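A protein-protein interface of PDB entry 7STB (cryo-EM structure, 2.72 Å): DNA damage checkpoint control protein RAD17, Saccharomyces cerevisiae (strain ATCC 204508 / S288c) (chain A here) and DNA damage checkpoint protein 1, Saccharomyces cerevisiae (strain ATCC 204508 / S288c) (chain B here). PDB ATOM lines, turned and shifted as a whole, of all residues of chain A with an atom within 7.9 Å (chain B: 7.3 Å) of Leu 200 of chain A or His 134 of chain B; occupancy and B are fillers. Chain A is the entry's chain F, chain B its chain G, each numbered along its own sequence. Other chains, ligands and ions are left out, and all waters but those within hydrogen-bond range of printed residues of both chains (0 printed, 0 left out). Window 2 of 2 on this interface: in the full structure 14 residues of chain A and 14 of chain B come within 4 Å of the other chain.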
ATOM      1  N   GLU A 172       4.694  -7.902   5.528  1.00  0.00           N
ATOM      2  CA  GLU A 172       4.087  -7.251   6.685  1.00  0.00           C
ATOM      3  C   GLU A 172       3.783  -8.252   7.794  1.00  0.00           C
ATOM      4  O   GLU A 172       3.982  -7.955   8.978  1.00  0.00           O
ATOM      5  CB  GLU A 172       2.815  -6.517   6.260  1.00  0.00           C
ATOM      6  CG  GLU A 172       2.063  -5.845   7.402  1.00  0.00           C
ATOM      7  CD  GLU A 172       2.911  -4.837   8.154  1.00  0.00           C
ATOM      8  OE1 GLU A 172       3.825  -4.248   7.539  1.00  0.00           O
ATOM      9  OE2 GLU A 172       2.662  -4.633   9.361  1.00  0.00           O
ATOM     10  N   ILE A 173       3.307  -9.444   7.435  1.00  0.00           N
ATOM     11  CA  ILE A 173       2.861 -10.421   8.424  1.00  0.00           C
ATOM     12  C   ILE A 173       4.040 -11.225   8.958  1.00  0.00           C
ATOM     13  O   ILE A 173       3.853 -12.195   9.700  1.00  0.00           O
ATOM     14  CB  ILE A 173       1.787 -11.356   7.834  1.00  0.00           C
ATOM     15  CG1 ILE A 173       2.372 -12.228   6.718  1.00  0.00           C
ATOM     16  CG2 ILE A 173       0.610 -10.543   7.314  1.00  0.00           C
ATOM     17  CD1 ILE A 173       1.392 -13.234   6.158  1.00  0.00           C
ATOM     18  N   GLY A 174       5.258 -10.835   8.592  1.00  0.00           N
ATOM     19  CA  GLY A 174       6.434 -11.535   9.069  1.00  0.00           C
ATOM     20  C   GLY A 174       6.506 -12.967   8.582  1.00  0.00           C
ATOM     21  O   GLY A 174       6.756 -13.886   9.368  1.00  0.00           O
ATOM     22  N   CYS A 175       6.280 -13.168   7.286  1.00  0.00           N
ATOM     23  CA  CYS A 175       6.291 -14.510   6.722  1.00  0.00           C
ATOM     24  C   CYS A 175       7.623 -15.198   6.990  1.00  0.00           C
ATOM     25  O   CYS A 175       8.691 -14.589   6.890  1.00  0.00           O
ATOM     26  CB  CYS A 175       6.028 -14.451   5.217  1.00  0.00           C
ATOM     27  SG  CYS A 175       5.941 -16.066   4.413  1.00  0.00           S
ATOM     28  N   SER A 196       1.677 -18.571   2.927  1.00  0.00           N
ATOM     29  CA  SER A 196       2.688 -18.147   3.884  1.00  0.00           C
ATOM     30  C   SER A 196       2.477 -18.854   5.213  1.00  0.00           C
ATOM     31  O   SER A 196       1.371 -18.837   5.764  1.00  0.00           O
ATOM     32  CB  SER A 196       2.643 -16.631   4.085  1.00  0.00           C
ATOM     33  OG  SER A 196       3.608 -16.218   5.036  1.00  0.00           O
ATOM     34  N   LYS A 197       3.539 -19.477   5.717  1.00  0.00           N
ATOM     35  CA  LYS A 197       3.575 -20.026   7.066  1.00  0.00           C
ATOM     36  C   LYS A 197       4.353 -19.055   7.944  1.00  0.00           C
ATOM     37  O   LYS A 197       5.533 -18.785   7.686  1.00  0.00           O
ATOM     38  CB  LYS A 197       4.223 -21.409   7.083  1.00  0.00           C
ATOM     39  CG  LYS A 197       4.032 -22.171   8.388  1.00  0.00           C
ATOM     40  CD  LYS A 197       5.169 -21.925   9.365  1.00  0.00           C
ATOM     41  CE  LYS A 197       4.960 -22.694  10.658  1.00  0.00           C
ATOM     42  NZ  LYS A 197       6.029 -22.417  11.656  1.00  0.00           N
ATOM     43  N   SER A 198       3.691 -18.536   8.975  1.00  0.00           N
ATOM     44  CA  SER A 198       4.266 -17.499   9.822  1.00  0.00           C
ATOM     45  C   SER A 198       3.673 -17.620  11.222  1.00  0.00           C
ATOM     46  O   SER A 198       3.002 -18.603  11.550  1.00  0.00           O
ATOM     47  CB  SER A 198       4.011 -16.114   9.215  1.00  0.00           C
ATOM     48  OG  SER A 198       2.689 -15.678   9.483  1.00  0.00           O
ATOM     49  N   GLN A 199       3.926 -16.604  12.053  1.00  0.00           N
ATOM     50  CA  GLN A 199       3.345 -16.578  13.391  1.00  0.00           C
ATOM     51  C   GLN A 199       1.827 -16.466  13.334  1.00  0.00           C
ATOM     52  O   GLN A 199       1.141 -16.834  14.293  1.00  0.00           O
ATOM     53  CB  GLN A 199       3.936 -15.418  14.192  1.00  0.00           C
ATOM     54  CG  GLN A 199       5.452 -15.457  14.302  1.00  0.00           C
ATOM     55  CD  GLN A 199       5.961 -14.893  15.615  1.00  0.00           C
ATOM     56  OE1 GLN A 199       6.421 -15.633  16.484  1.00  0.00           O
ATOM     57  NE2 GLN A 199       5.883 -13.576  15.763  1.00  0.00           N
ATOM     58  N   LEU A 200       1.289 -15.959  12.223  1.00  0.00           N
ATOM     59  CA  LEU A 200      -0.151 -15.938  12.011  1.00  0.00           C
ATOM     60  C   LEU A 200      -0.726 -17.322  11.763  1.00  0.00           C
ATOM     61  O   LEU A 200      -1.951 -17.480  11.790  1.00  0.00           O
ATOM     62  CB  LEU A 200      -0.489 -15.035  10.822  1.00  0.00           C
ATOM     63  CG  LEU A 200      -0.601 -13.534  11.088  1.00  0.00           C
ATOM     64  CD1 LEU A 200      -1.753 -13.260  12.029  1.00  0.00           C
ATOM     65  CD2 LEU A 200       0.699 -12.979  11.648  1.00  0.00           C
ATOM     66  N   GLY A 201       0.117 -18.315  11.522  1.00  0.00           N
ATOM     67  CA  GLY A 201      -0.342 -19.629  11.107  1.00  0.00           C
ATOM     68  C   GLY A 201      -0.094 -19.845   9.620  1.00  0.00           C
ATOM     69  O   GLY A 201       1.036 -19.721   9.150  1.00  0.00           O
ATOM     70  N   PHE A 202      -1.159 -20.152   8.884  1.00  0.00           N
ATOM     71  CA  PHE A 202      -1.101 -20.346   7.441  1.00  0.00           C
ATOM     72  C   PHE A 202      -2.061 -19.371   6.775  1.00  0.00           C
ATOM     73  O   PHE A 202      -3.265 -19.394   7.053  1.00  0.00           O
ATOM     74  CB  PHE A 202      -1.456 -21.786   7.066  1.00  0.00           C
ATOM     75  CG  PHE A 202      -0.296 -22.736   7.145  1.00  0.00           C
ATOM     76  CD1 PHE A 202       0.467 -23.010   6.025  1.00  0.00           C
ATOM     77  CD2 PHE A 202       0.031 -23.353   8.340  1.00  0.00           C
ATOM     78  CE1 PHE A 202       1.532 -23.883   6.092  1.00  0.00           C
ATOM     79  CE2 PHE A 202       1.096 -24.228   8.415  1.00  0.00           C
ATOM     80  CZ  PHE A 202       1.848 -24.494   7.289  1.00  0.00           C
ATOM     81  N   SER A 203      -1.530 -18.523   5.900  1.00  0.00           N
ATOM     82  CA  SER A 203      -2.326 -17.570   5.141  1.00  0.00           C
ATOM     83  C   SER A 203      -2.159 -17.849   3.654  1.00  0.00           C
ATOM     84  O   SER A 203      -1.154 -18.417   3.226  1.00  0.00           O
ATOM     85  CB  SER A 203      -1.920 -16.126   5.460  1.00  0.00           C
ATOM     86  OG  SER A 203      -0.578 -15.879   5.082  1.00  0.00           O
ATOM     87  N   ILE B  54      -9.300  -1.607  16.631  1.00  0.00           N
ATOM     88  CA  ILE B  54      -8.533  -2.810  16.941  1.00  0.00           C
ATOM     89  C   ILE B  54      -7.132  -2.439  17.411  1.00  0.00           C
ATOM     90  O   ILE B  54      -6.598  -3.039  18.350  1.00  0.00           O
ATOM     91  CB  ILE B  54      -8.496  -3.751  15.722  1.00  0.00           C
ATOM     92  CG1 ILE B  54      -9.903  -4.261  15.390  1.00  0.00           C
ATOM     93  CG2 ILE B  54      -7.556  -4.920  15.977  1.00  0.00           C
ATOM     94  CD1 ILE B  54     -10.577  -5.041  16.504  1.00  0.00           C
ATOM     95  N   SER B  58      -5.610  -3.330  21.063  1.00  0.00           N
ATOM     96  CA  SER B  58      -4.330  -4.013  21.202  1.00  0.00           C
ATOM     97  C   SER B  58      -3.344  -3.178  22.006  1.00  0.00           C
ATOM     98  O   SER B  58      -2.424  -3.727  22.624  1.00  0.00           O
ATOM     99  CB  SER B  58      -3.754  -4.337  19.822  1.00  0.00           C
ATOM    100  OG  SER B  58      -3.298  -3.167  19.170  1.00  0.00           O
ATOM    101  N   ASP B  62      -2.732  -7.042  25.453  1.00  0.00           N
ATOM    102  CA  ASP B  62      -2.100  -7.867  24.427  1.00  0.00           C
ATOM    103  C   ASP B  62      -3.124  -8.722  23.688  1.00  0.00           C
ATOM    104  O   ASP B  62      -3.025  -8.901  22.470  1.00  0.00           O
ATOM    105  CB  ASP B  62      -1.016  -8.744  25.054  1.00  0.00           C
ATOM    106  CG  ASP B  62      -1.581  -9.807  25.977  1.00  0.00           C
ATOM    107  OD1 ASP B  62      -2.762  -9.696  26.367  1.00  0.00           O
ATOM    108  OD2 ASP B  62      -0.841 -10.754  26.314  1.00  0.00           O
ATOM    109  N   ASP B  63      -4.105  -9.261  24.404  1.00  0.00           N
ATOM    110  CA  ASP B  63      -5.166 -10.067  23.816  1.00  0.00           C
ATOM    111  C   ASP B  63      -6.482  -9.304  23.895  1.00  0.00           C
ATOM    112  O   ASP B  63      -6.872  -8.842  24.972  1.00  0.00           O
ATOM    113  CB  ASP B  63      -5.294 -11.412  24.533  1.00  0.00           C
ATOM    114  CG  ASP B  63      -4.133 -12.346  24.242  1.00  0.00           C
ATOM    115  OD1 ASP B  63      -3.630 -12.338  23.100  1.00  0.00           O
ATOM    116  OD2 ASP B  63      -3.726 -13.091  25.157  1.00  0.00           O
ATOM    117  N   VAL B 130      -8.456 -13.190  21.185  1.00  0.00           N
ATOM    118  CA  VAL B 130      -7.603 -13.212  20.003  1.00  0.00           C
ATOM    119  C   VAL B 130      -6.432 -12.268  20.224  1.00  0.00           C
ATOM    120  O   VAL B 130      -6.601 -11.169  20.761  1.00  0.00           O
ATOM    121  CB  VAL B 130      -8.381 -12.810  18.731  1.00  0.00           C
ATOM    122  CG1 VAL B 130      -7.540 -13.070  17.492  1.00  0.00           C
ATOM    123  CG2 VAL B 130      -9.697 -13.559  18.652  1.00  0.00           C
ATOM    124  N   ASN B 131      -5.245 -12.692  19.801  1.00  0.00           N
ATOM    125  CA  ASN B 131      -4.077 -11.825  19.874  1.00  0.00           C
ATOM    126  C   ASN B 131      -4.356 -10.514  19.147  1.00  0.00           C
ATOM    127  O   ASN B 131      -4.668 -10.508  17.952  1.00  0.00           O
ATOM    128  CB  ASN B 131      -2.866 -12.531  19.269  1.00  0.00           C
ATOM    129  CG  ASN B 131      -1.609 -11.692  19.338  1.00  0.00           C
ATOM    130  OD1 ASN B 131      -1.542 -10.604  18.771  1.00  0.00           O
ATOM    131  ND2 ASN B 131      -0.602 -12.195  20.038  1.00  0.00           N
ATOM    132  N   GLY B 132      -4.248  -9.402  19.876  1.00  0.00           N
ATOM    133  CA  GLY B 132      -4.566  -8.109  19.292  1.00  0.00           C
ATOM    134  C   GLY B 132      -3.599  -7.697  18.198  1.00  0.00           C
ATOM    135  O   GLY B 132      -4.003  -7.104  17.194  1.00  0.00           O
ATOM    136  N   ARG B 133      -2.311  -7.995  18.379  1.00  0.00           N
ATOM    137  CA  ARG B 133      -1.321  -7.607  17.380  1.00  0.00           C
ATOM    138  C   ARG B 133      -1.603  -8.270  16.037  1.00  0.00           C
ATOM    139  O   ARG B 133      -1.505  -7.625  14.987  1.00  0.00           O
ATOM    140  CB  ARG B 133       0.084  -7.962  17.868  1.00  0.00           C
ATOM    141  CG  ARG B 133       0.556  -7.126  19.043  1.00  0.00           C
ATOM    142  CD  ARG B 133       2.056  -7.244  19.249  1.00  0.00           C
ATOM    143  NE  ARG B 133       2.553  -8.578  18.937  1.00  0.00           N
ATOM    144  CZ  ARG B 133       2.506  -9.612  19.768  1.00  0.00           C
ATOM    145  NH1 ARG B 133       1.985  -9.504  20.980  1.00  0.00           N
ATOM    146  NH2 ARG B 133       2.994 -10.784  19.373  1.00  0.00           N
ATOM    147  N   HIS B 134      -1.946  -9.560  16.049  1.00  0.00           N
ATOM    148  CA  HIS B 134      -2.246 -10.250  14.800  1.00  0.00           C
ATOM    149  C   HIS B 134      -3.479  -9.666  14.122  1.00  0.00           C
ATOM    150  O   HIS B 134      -3.488  -9.466  12.901  1.00  0.00           O
ATOM    151  CB  HIS B 134      -2.437 -11.745  15.057  1.00  0.00           C
ATOM    152  CG  HIS B 134      -1.228 -12.420  15.625  1.00  0.00           C
ATOM    153  ND1 HIS B 134      -1.308 -13.505  16.471  1.00  0.00           N
ATOM    154  CD2 HIS B 134       0.092 -12.158  15.473  1.00  0.00           C
ATOM    155  CE1 HIS B 134      -0.090 -13.886  16.810  1.00  0.00           C
ATOM    156  NE2 HIS B 134       0.778 -13.085  16.220  1.00  0.00           N
ATOM    157  N   LEU B 135      -4.530  -9.386  14.891  1.00  0.00           N
ATOM    158  CA  LEU B 135      -5.730  -8.805  14.297  1.00  0.00           C
ATOM    159  C   LEU B 135      -5.430  -7.438  13.697  1.00  0.00           C
ATOM    160  O   LEU B 135      -5.920  -7.105  12.611  1.00  0.00           O
ATOM    161  CB  LEU B 135      -6.839  -8.709  15.344  1.00  0.00           C
ATOM    162  CG  LEU B 135      -8.261  -8.485  14.822  1.00  0.00           C
ATOM    163  CD1 LEU B 135      -8.664  -9.558  13.821  1.00  0.00           C
ATOM    164  CD2 LEU B 135      -9.247  -8.438  15.976  1.00  0.00           C
ATOM    165  N   THR B 136      -4.624  -6.631  14.390  1.00  0.00           N
ATOM    166  CA  THR B 136      -4.249  -5.327  13.854  1.00  0.00           C
ATOM    167  C   THR B 136      -3.441  -5.470  12.570  1.00  0.00           C
ATOM    168  O   THR B 136      -3.687  -4.755  11.591  1.00  0.00           O
ATOM    169  CB  THR B 136      -3.458  -4.542  14.900  1.00  0.00           C
ATOM    170  OG1 THR B 136      -4.215  -4.458  16.112  1.00  0.00           O
ATOM    171  CG2 THR B 136      -3.156  -3.138  14.400  1.00  0.00           C
ATOM    172  N   THR B 137      -2.472  -6.389  12.552  1.00  0.00           N
ATOM    173  CA  THR B 137      -1.668  -6.605  11.354  1.00  0.00           C
ATOM    174  C   THR B 137      -2.472  -7.237  10.227  1.00  0.00           C
ATOM    175  O   THR B 137      -2.010  -7.244   9.082  1.00  0.00           O
ATOM    176  CB  THR B 137      -0.460  -7.486  11.681  1.00  0.00           C
ATOM    177  OG1 THR B 137       0.197  -6.988  12.851  1.00  0.00           O
ATOM    178  CG2 THR B 137       0.523  -7.502  10.520  1.00  0.00           C
ATOM    179  N   ILE B 138      -3.641  -7.794  10.528  1.00  0.00           N
ATOM    180  CA  ILE B 138      -4.516  -8.301   9.478  1.00  0.00           C
ATOM    181  C   ILE B 138      -5.479  -7.227   8.977  1.00  0.00           C
ATOM    182  O   ILE B 138      -5.905  -7.273   7.818  1.00  0.00           O
ATOM    183  CB  ILE B 138      -5.284  -9.535   9.981  1.00  0.00           C
ATOM    184  CG1 ILE B 138      -4.346 -10.740  10.076  1.00  0.00           C
ATOM    185  CG2 ILE B 138      -6.460  -9.847   9.062  1.00  0.00           C
ATOM    186  CD1 ILE B 138      -4.941 -11.927  10.802  1.00  0.00           C
ATOM    187  N   SER B 139      -5.833  -6.258   9.822  1.00  0.00           N
ATOM    188  CA  SER B 139      -6.832  -5.257   9.472  1.00  0.00           C
ATOM    189  C   SER B 139      -6.243  -3.989   8.866  1.00  0.00           C
ATOM    190  O   SER B 139      -7.009  -3.114   8.448  1.00  0.00           O
ATOM    191  CB  SER B 139      -7.650  -4.881  10.713  1.00  0.00           C
ATOM    192  OG  SER B 139      -8.290  -6.017  11.265  1.00  0.00           O
ATOM    193  N   ARG B 140      -4.920  -3.860   8.803  1.00  0.00           N
ATOM    194  CA  ARG B 140      -4.322  -2.628   8.303  1.00  0.00           C
ATOM    195  C   ARG B 140      -4.579  -2.466   6.808  1.00  0.00           C
ATOM    196  O   ARG B 140      -4.647  -3.440   6.054  1.00  0.00           O
ATOM    197  CB  ARG B 140      -2.818  -2.603   8.588  1.00  0.00           C
ATOM    198  CG  ARG B 140      -1.943  -3.281   7.540  1.00  0.00           C
ATOM    199  CD  ARG B 140      -2.238  -4.763   7.457  1.00  0.00           C
ATOM    200  NE  ARG B 140      -1.321  -5.466   6.567  1.00  0.00           N
ATOM    201  CZ  ARG B 140      -1.479  -5.572   5.254  1.00  0.00           C
ATOM    202  NH1 ARG B 140      -2.512  -5.025   4.634  1.00  0.00           N
ATOM    203  NH2 ARG B 140      -0.578  -6.246   4.545  1.00  0.00           N
ATOM    204  N   ARG B 167     -10.520 -21.302  15.059  1.00  0.00           N
ATOM    205  CA  ARG B 167      -9.778 -20.359  14.235  1.00  0.00           C
ATOM    206  C   ARG B 167     -10.743 -19.354  13.626  1.00  0.00           C
ATOM    207  O   ARG B 167     -11.811 -19.725  13.130  1.00  0.00           O
ATOM    208  CB  ARG B 167      -9.000 -21.080  13.130  1.00  0.00           C
ATOM    209  CG  ARG B 167      -7.663 -21.635  13.585  1.00  0.00           C
ATOM    210  CD  ARG B 167      -6.912 -22.284  12.439  1.00  0.00           C
ATOM    211  NE  ARG B 167      -5.872 -23.192  12.911  1.00  0.00           N
ATOM    212  CZ  ARG B 167      -4.693 -22.805  13.377  1.00  0.00           C
ATOM    213  NH1 ARG B 167      -4.364 -21.525  13.455  1.00  0.00           N
ATOM    214  NH2 ARG B 167      -3.821 -23.725  13.778  1.00  0.00           N
ATOM    215  N   TYR B 182      -6.795 -15.555   6.193  1.00  0.00           N
ATOM    216  CA  TYR B 182      -6.124 -15.686   7.480  1.00  0.00           C
ATOM    217  C   TYR B 182      -6.988 -16.511   8.422  1.00  0.00           C
ATOM    218  O   TYR B 182      -8.219 -16.402   8.405  1.00  0.00           O
ATOM    219  CB  TYR B 182      -5.847 -14.318   8.116  1.00  0.00           C
ATOM    220  CG  TYR B 182      -5.050 -13.369   7.253  1.00  0.00           C
ATOM    221  CD1 TYR B 182      -3.663 -13.380   7.272  1.00  0.00           C
ATOM    222  CD2 TYR B 182      -5.686 -12.452   6.429  1.00  0.00           C
ATOM    223  CE1 TYR B 182      -2.932 -12.509   6.490  1.00  0.00           C
ATOM    224  CE2 TYR B 182      -4.965 -11.577   5.643  1.00  0.00           C
ATOM    225  CZ  TYR B 182      -3.588 -11.610   5.677  1.00  0.00           C
ATOM    226  OH  TYR B 182      -2.864 -10.741   4.896  1.00  0.00           O
ATOM    227  N   CYS B 183      -6.342 -17.339   9.244  1.00  0.00           N
ATOM    228  CA  CYS B 183      -7.029 -18.152  10.249  1.00  0.00           C
ATOM    229  C   CYS B 183      -6.274 -18.074  11.570  1.00  0.00           C
ATOM    230  O   CYS B 183      -5.690 -19.060  12.033  1.00  0.00           O
ATOM    231  CB  CYS B 183      -7.165 -19.600   9.774  1.00  0.00           C
ATOM    232  SG  CYS B 183      -5.629 -20.336   9.177  1.00  0.00           S
ATOM    233  N   PRO B 184      -6.261 -16.904  12.206  1.00  0.00           N
ATOM    234  CA  PRO B 184      -5.634 -16.794  13.529  1.00  0.00           C
ATOM    235  C   PRO B 184      -6.407 -17.552  14.600  1.00  0.00           C
ATOM    236  O   PRO B 184      -7.632 -17.691  14.544  1.00  0.00           O
ATOM    237  CB  PRO B 184      -5.639 -15.284  13.801  1.00  0.00           C
ATOM    238  CG  PRO B 184      -6.700 -14.734  12.909  1.00  0.00           C
ATOM    239  CD  PRO B 184      -6.682 -15.592  11.687  1.00  0.00           C
ATOM    240  N   GLN B 185      -5.669 -18.029  15.598  1.00  0.00           N
ATOM    241  CA  GLN B 185      -6.267 -18.795  16.683  1.00  0.00           C
ATOM    242  C   GLN B 185      -7.075 -17.896  17.612  1.00  0.00           C
ATOM    243  O   GLN B 185      -6.714 -16.741  17.853  1.00  0.00           O
ATOM    244  CB  GLN B 185      -5.180 -19.509  17.486  1.00  0.00           C
ATOM    245  CG  GLN B 185      -4.401 -20.545  16.701  1.00  0.00           C
ATOM    246  CD  GLN B 185      -3.089 -20.914  17.368  1.00  0.00           C
ATOM    247  OE1 GLN B 185      -2.666 -20.272  18.331  1.00  0.00           O
ATOM    248  NE2 GLN B 185      -2.439 -21.953  16.859  1.00  0.00           N
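The backbone carbonyl oxygen of Phe 202 of chain A lies within hydrogen-bond range of the side-chain sulfur of Cys 183 of chain B, at 3.3 Å.
The side-chain hydroxyl of Ser 198 of chain A sits close to the backbone NH of Leu 200 of chain A (3.1 Å). The backbone NH (N) of His 134 of chain B is in hydrogen-bond range of the side-chain amide oxygen (OD1) of Asn 131 of chain B (2.9 Å). OG1 of Thr 137 of chain B lies within hydrogen-bond range of O of Arg 133 of chain B (2.8 Å). O of Ser 203 of chain A lies within hydrogen-bond range of N of Ser 196 of chain A (2.9 Å). The backbone carbonyl oxygen (O) of Cys 183 of chain B is in hydrogen-bond range of the guanidinium group (NH1) of Arg 167 of chain B (3.1 Å). NE of Arg 140 of chain B lies close to O of Thr 137 of chain B.
Glu 172 of chain A touches Thr 137 of chain B (OE2 to CG2, 3.8 Å). Glu 172 of chain A touches Arg 140 of chain B (CG to NE, 3.5 Å). Leu 200 of chain A touches His 134 of chain B (CD1 to CB, 3.5 Å). Leu 200 of chain A touches Ile 138 of chain B (CD1 to CD1, 3.7 Å). Tyr 182 of chain B touches Ser 203 of chain A.
Of chain B, only His 134 and Ile 138 come within 4 Å of Leu 200 of chain A. Of chain A, only Leu 200 comes within 4 Å of His 134 of chain B. Printed residues of chain B within 4 Å of Ser 203 of chain A: Tyr 182. Of the printed residues of chain A, Cys 183 of chain B touches Phe 202 (3.3 Å). Of the printed residues of chain A, Ile 138 of chain B touches Leu 200. The nearest printed residue of chain B that does not touch Phe 202 of chain A is Tyr 182 of chain B (4.7 Å).
Hydrophobic or aromatic side chains of chain A within 4 Å of the printed part of chain B: Leu 200. Among the printed residues, 6 pairs touch across the chains. Among the printed residues, no Asp or Glu carboxylate lies within 4 Å of a Lys or Arg side-chain nitrogen of the other chain.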
